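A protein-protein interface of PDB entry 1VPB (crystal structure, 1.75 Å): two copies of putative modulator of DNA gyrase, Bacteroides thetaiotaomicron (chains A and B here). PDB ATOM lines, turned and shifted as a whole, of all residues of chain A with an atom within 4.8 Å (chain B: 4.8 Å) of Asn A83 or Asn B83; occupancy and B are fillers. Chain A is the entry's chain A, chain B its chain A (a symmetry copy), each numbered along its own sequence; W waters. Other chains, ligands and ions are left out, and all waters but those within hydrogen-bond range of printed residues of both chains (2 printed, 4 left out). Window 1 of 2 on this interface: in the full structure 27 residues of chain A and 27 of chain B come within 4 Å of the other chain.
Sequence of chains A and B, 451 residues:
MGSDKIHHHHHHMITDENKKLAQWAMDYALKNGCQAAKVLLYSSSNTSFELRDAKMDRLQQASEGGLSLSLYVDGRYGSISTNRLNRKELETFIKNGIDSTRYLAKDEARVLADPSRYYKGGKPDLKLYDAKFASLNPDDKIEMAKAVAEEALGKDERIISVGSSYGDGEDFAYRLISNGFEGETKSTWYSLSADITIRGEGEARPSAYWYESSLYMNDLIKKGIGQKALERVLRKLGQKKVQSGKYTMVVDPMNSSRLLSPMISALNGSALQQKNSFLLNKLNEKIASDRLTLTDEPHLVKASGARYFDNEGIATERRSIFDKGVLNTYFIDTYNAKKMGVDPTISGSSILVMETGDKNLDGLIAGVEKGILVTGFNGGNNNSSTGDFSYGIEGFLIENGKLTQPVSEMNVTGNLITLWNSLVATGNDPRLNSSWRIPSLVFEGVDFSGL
The backbone carbonyl oxygen (O) of Glu A64 is in hydrogen-bond range of the guanidinium group (NH1) of Arg B84, 3.4 Å away. The guanidinium group (NH1) of Arg A84 lies within hydrogen-bond range of the backbone carbonyl oxygen (O) of Glu B64, at 3.4 Å. The side-chain hydroxyl (OG1) of Thr A82 lies within hydrogen-bond range of the backbone carbonyl oxygen (O) of Ser B63, at 3.0 Å. The backbone NH (N) of Gly B65 sits at hydrogen-bond distance from the side-chain amide oxygen (OD1) of Asn A83, at 2.8 Å. N of Gly A65 sits at hydrogen-bond distance from OD1 of Asn B83 (2.8 Å). O of Ser A81 is in hydrogen-bond range of N of Ser B63. The backbone NH (N) of Asn A83 sits at hydrogen-bond distance from the backbone carbonyl oxygen (O) of Ser B63 (3.2 Å). The side-chain amide nitrogen of Asn A83 lies close to the side-chain amide nitrogen of Asn B83 (2.9 Å). The backbone carbonyl oxygen of Ser B81 is in hydrogen-bond range of the backbone NH of Ser A63, 3.1 Å away. N of Asn B83 is in hydrogen-bond range of O of Ser A63 (3.2 Å). O of Ser A63 lies within hydrogen-bond range of OG1 of Thr B82, 3.0 Å away.
The side-chain hydroxyl (OG1) of Thr A82 is in hydrogen-bond range of the backbone NH (N) of Arg A84, 3.0 Å away. The side-chain hydroxyl (OG1) of Thr B82 sits at hydrogen-bond distance from the backbone NH (N) of Arg B84 (3.0 Å).
Ser A63 touches Arg B84 (OG to CD, 3.2 Å). Glu A64 touches Asn B83. Arg B84 touches Gly A65 (NH1 to CA, 3.3 Å). Asn A83 touches Glu B64. Ser B63 touches Arg A84 (OG to CD, 3.2 Å). Gly B65 touches Arg A84.
Printed residues of chain B within 4 Å of Gly A65: Asn B83 and Arg B84. Of the printed residues of chain B, Ser A81 touches Ser B63 (3.1 Å). Of the printed residues of chain A, Glu B64 touches Asn A83 (3.2 Å) and Arg A84 (3.4 Å). Of the printed residues of chain A, Ser B81 touches Ser A63. Of chain A, only Ser A63, Glu A64, Gly A65 and Asn A83 come within 4 Å of Asn B83. The nearest printed residue of chain B that does not touch Asn A83 is Gly B66 (5.3 Å). The nearest printed residue of chain A that does not touch Asn B83 is Gly A66 (5.3 Å). The nearest printed residue of chain B that does not touch Glu A64 is Thr B82 (5.0 Å).
Of the 9 printed residues of chain B, 7 touch a printed residue of chain A. Among the printed residues, 17 pairs touch across the chains.
Glu A64 touches Asn B83, and with the chains exchanged Asn A83 touches Glu B64. Glu A64 touches Arg B84, and with the chains exchanged Arg A84 touches Glu B64. Gly A65 touches Arg B84, and with the chains exchanged Arg A84 touches Gly B65. Asn A83 touches its own counterpart, Asn B83. Positions printed for both chains: 63, 64, 65, 66, 81, 82, 83, 84 and 85.
Water W1 lies within hydrogen-bond range of the side-chain hydroxyl (OG) of Ser A63 (2.8 Å) and the guanidinium group (NE) of Arg B84 (3.4 Å). Water W2 lies within hydrogen-bond range of OG of Ser B63 (2.8 Å) and NE of Arg A84 (3.4 Å).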
ATOM      1  N   SER A  63      25.504  35.106  32.825  1.00  0.00           N
ATOM      2  CA  SER A  63      26.684  34.990  32.003  1.00  0.00           C
ATOM      3  C   SER A  63      26.292  34.202  30.762  1.00  0.00           C
ATOM      4  O   SER A  63      25.763  33.109  30.879  1.00  0.00           O
ATOM      5  CB  SER A  63      27.749  34.223  32.702  1.00  0.00           C
ATOM      6  OG  SER A  63      28.909  34.232  31.928  1.00  0.00           O
ATOM      7  N   GLU A  64      26.479  34.769  29.593  1.00  0.00           N
ATOM      8  CA  GLU A  64      25.893  34.114  28.397  1.00  0.00           C
ATOM      9  C   GLU A  64      26.926  34.152  27.293  1.00  0.00           C
ATOM     10  O   GLU A  64      27.812  35.011  27.282  1.00  0.00           O
ATOM     11  CB  GLU A  64      24.607  34.844  27.980  1.00  0.00           C
ATOM     12  CG  GLU A  64      23.472  34.933  28.986  1.00  0.00           C
ATOM     13  N   GLY A  65      26.872  33.178  26.376  1.00  0.00           N
ATOM     14  CA  GLY A  65      27.739  33.180  25.221  1.00  0.00           C
ATOM     15  C   GLY A  65      27.101  32.351  24.152  1.00  0.00           C
ATOM     16  O   GLY A  65      26.531  31.293  24.487  1.00  0.00           O
ATOM     17  N   GLY A  66      27.181  32.798  22.914  1.00  0.00           N
ATOM     18  CA  GLY A  66      26.610  31.995  21.838  1.00  0.00           C
ATOM     19  C   GLY A  66      27.189  32.267  20.462  1.00  0.00           C
ATOM     20  O   GLY A  66      28.128  33.062  20.288  1.00  0.00           O
ATOM     21  N   SER A  81      20.900  30.302  15.459  1.00  0.00           N
ATOM     22  CA  SER A  81      21.664  30.746  16.619  1.00  0.00           C
ATOM     23  C   SER A  81      21.597  29.698  17.703  1.00  0.00           C
ATOM     24  O   SER A  81      20.549  29.057  17.885  1.00  0.00           O
ATOM     25  CB  SER A  81      21.078  32.069  17.092  1.00  0.00           C
ATOM     26  OG  SER A  81      19.831  31.847  17.735  1.00  0.00           O
ATOM     27  N   THR A  82      22.731  29.479  18.384  1.00  0.00           N
ATOM     28  CA  THR A  82      22.831  28.477  19.398  1.00  0.00           C
ATOM     29  C   THR A  82      23.822  28.844  20.476  1.00  0.00           C
ATOM     30  O   THR A  82      24.787  29.618  20.250  1.00  0.00           O
ATOM     31  CB  THR A  82      23.257  27.175  18.754  1.00  0.00           C
ATOM     32  OG1 THR A  82      23.272  26.141  19.709  1.00  0.00           O
ATOM     33  CG2 THR A  82      24.658  27.268  18.106  1.00  0.00           C
ATOM     34  N   ASN A  83      23.569  28.301  21.660  1.00  0.00           N
ATOM     35  CA  ASN A  83      24.562  28.427  22.701  1.00  0.00           C
ATOM     36  C   ASN A  83      25.074  27.091  23.114  1.00  0.00           C
ATOM     37  O   ASN A  83      25.665  26.978  24.183  1.00  0.00           O
ATOM     38  CB  ASN A  83      24.027  29.229  23.867  1.00  0.00           C
ATOM     39  CG  ASN A  83      22.790  28.620  24.508  1.00  0.00           C
ATOM     40  OD1 ASN A  83      22.604  27.400  24.497  1.00  0.00           O
ATOM     41  ND2 ASN A  83      21.990  29.475  25.174  1.00  0.00           N
ATOM     42  N   ARG A  84      24.802  26.065  22.303  1.00  0.00           N
ATOM     43  CA  ARG A  84      25.210  24.717  22.568  1.00  0.00           C
ATOM     44  C   ARG A  84      26.364  24.415  21.640  1.00  0.00           C
ATOM     45  O   ARG A  84      26.154  24.055  20.486  1.00  0.00           O
ATOM     46  CB  ARG A  84      24.065  23.705  22.351  1.00  0.00           C
ATOM     47  CG  ARG A  84      22.862  23.953  23.196  1.00  0.00           C
ATOM     48  CD  ARG A  84      21.695  23.005  22.898  1.00  0.00           C
ATOM     49  NE  ARG A  84      21.843  21.677  23.439  1.00  0.00           N
ATOM     50  CZ  ARG A  84      21.516  21.331  24.675  1.00  0.00           C
ATOM     51  NH1 ARG A  84      21.098  22.240  25.538  1.00  0.00           N
ATOM     52  NH2 ARG A  84      21.662  20.088  25.085  1.00  0.00           N
ATOM     53  N   LEU A  85      27.584  24.520  22.169  1.00  0.00           N
ATOM     54  CA  LEU A  85      28.782  24.695  21.347  1.00  0.00           C
ATOM     55  C   LEU A  85      29.755  23.537  21.213  1.00  0.00           C
ATOM     56  O   LEU A  85      30.855  23.761  20.726  1.00  0.00           O
ATOM     57  CB  LEU A  85      29.542  25.927  21.828  1.00  0.00           C
ATOM     58  CG  LEU A  85      28.708  27.207  21.876  1.00  0.00           C
ATOM     59  CD1 LEU A  85      29.541  28.436  22.195  1.00  0.00           C
ATOM     60  CD2 LEU A  85      27.930  27.435  20.569  1.00  0.00           C
ATOM     61  N   SER B  63      18.829  26.774  19.114  1.00  0.00           N
ATOM     62  CA  SER B  63      19.055  25.659  20.000  1.00  0.00           C
ATOM     63  C   SER B  63      19.720  26.207  21.254  1.00  0.00           C
ATOM     64  O   SER B  63      20.740  26.870  21.160  1.00  0.00           O
ATOM     65  CB  SER B  63      19.989  24.673  19.393  1.00  0.00           C
ATOM     66  OG  SER B  63      20.091  23.558  20.224  1.00  0.00           O
ATOM     67  N   GLU B  64      19.122  25.999  22.404  1.00  0.00           N
ATOM     68  CA  GLU B  64      19.633  26.721  23.597  1.00  0.00           C
ATOM     69  C   GLU B  64      19.673  25.743  24.749  1.00  0.00           C
ATOM     70  O   GLU B  64      18.937  24.752  24.767  1.00  0.00           O
ATOM     71  CB  GLU B  64      18.722  27.917  23.913  1.00  0.00           C
ATOM     72  CG  GLU B  64      18.538  28.982  22.847  1.00  0.00           C
ATOM     73  N   GLY B  65      20.583  25.966  25.705  1.00  0.00           N
ATOM     74  CA  GLY B  65      20.633  25.160  26.903  1.00  0.00           C
ATOM     75  C   GLY B  65      21.316  25.950  27.974  1.00  0.00           C
ATOM     76  O   GLY B  65      22.307  26.639  27.658  1.00  0.00           O
ATOM     77  N   GLY B  66      20.820  25.868  29.193  1.00  0.00           N
ATOM     78  CA  GLY B  66      21.486  26.588  30.273  1.00  0.00           C
ATOM     79  C   GLY B  66      21.220  26.041  31.664  1.00  0.00           C
ATOM     80  O   GLY B  66      20.546  25.014  31.850  1.00  0.00           O
ATOM     81  N   SER B  81      22.091  32.755  36.418  1.00  0.00           N
ATOM     82  CA  SER B  81      21.810  31.887  35.281  1.00  0.00           C
ATOM     83  C   SER B  81      22.896  32.043  34.244  1.00  0.00           C
ATOM     84  O   SER B  81      23.404  33.157  34.036  1.00  0.00           O
ATOM     85  CB  SER B  81      20.449  32.271  34.719  1.00  0.00           C
ATOM     86  OG  SER B  81      20.539  33.506  34.023  1.00  0.00           O
ATOM     87  N   THR B  82      23.295  30.918  33.632  1.00  0.00           N
ATOM     88  CA  THR B  82      24.352  30.905  32.672  1.00  0.00           C
ATOM     89  C   THR B  82      24.173  29.827  31.631  1.00  0.00           C
ATOM     90  O   THR B  82      23.521  28.779  31.871  1.00  0.00           O
ATOM     91  CB  THR B  82      25.664  30.685  33.394  1.00  0.00           C
ATOM     92  OG1 THR B  82      26.738  30.763  32.490  1.00  0.00           O
ATOM     93  CG2 THR B  82      25.720  29.315  34.109  1.00  0.00           C
ATOM     94  N   ASN B  83      24.739  30.096  30.460  1.00  0.00           N
ATOM     95  CA  ASN B  83      24.798  29.049  29.468  1.00  0.00           C
ATOM     96  C   ASN B  83      26.208  28.700  29.142  1.00  0.00           C
ATOM     97  O   ASN B  83      26.452  28.081  28.112  1.00  0.00           O
ATOM     98  CB  ASN B  83      23.994  29.420  28.240  1.00  0.00           C
ATOM     99  CG  ASN B  83      24.470  30.696  27.565  1.00  0.00           C
ATOM    100  OD1 ASN B  83      25.653  31.042  27.622  1.00  0.00           O
ATOM    101  ND2 ASN B  83      23.553  31.345  26.820  1.00  0.00           N
ATOM    102  N   ARG B  84      27.147  29.142  29.985  1.00  0.00           N
ATOM    103  CA  ARG B  84      28.549  28.904  29.802  1.00  0.00           C
ATOM    104  C   ARG B  84      28.949  27.843  30.801  1.00  0.00           C
ATOM    105  O   ARG B  84      29.219  28.151  31.958  1.00  0.00           O
ATOM    106  CB  ARG B  84      29.390  30.181  30.005  1.00  0.00           C
ATOM    107  CG  ARG B  84      29.032  31.301  29.089  1.00  0.00           C
ATOM    108  CD  ARG B  84      29.804  32.595  29.368  1.00  0.00           C
ATOM    109  NE  ARG B  84      31.166  32.600  28.896  1.00  0.00           N
ATOM    110  CZ  ARG B  84      31.530  32.914  27.662  1.00  0.00           C
ATOM    111  NH1 ARG B  84      30.620  33.168  26.739  1.00  0.00           N
ATOM    112  NH2 ARG B  84      32.801  32.914  27.318  1.00  0.00           N
ATOM    113  N   LEU B  85      29.030  26.597  30.332  1.00  0.00           N
ATOM    114  CA  LEU B  85      28.971  25.425  31.205  1.00  0.00           C
ATOM    115  C   LEU B  85      30.237  24.621  31.442  1.00  0.00           C
ATOM    116  O   LEU B  85      30.133  23.524  31.975  1.00  0.00           O
ATOM    117  CB  LEU B  85      27.874  24.488  30.710  1.00  0.00           C
ATOM    118  CG  LEU B  85      26.501  25.143  30.560  1.00  0.00           C
ATOM    119  CD1 LEU B  85      25.408  24.141  30.230  1.00  0.00           C
ATOM    120  CD2 LEU B  85      26.106  25.942  31.814  1.00  0.00           C
HETATM  121  O   HOH W   1      30.261  35.659  29.934  1.00  0.00           O
HETATM  122  O   HOH W   2      18.750  22.122  22.219  1.00  0.00           O
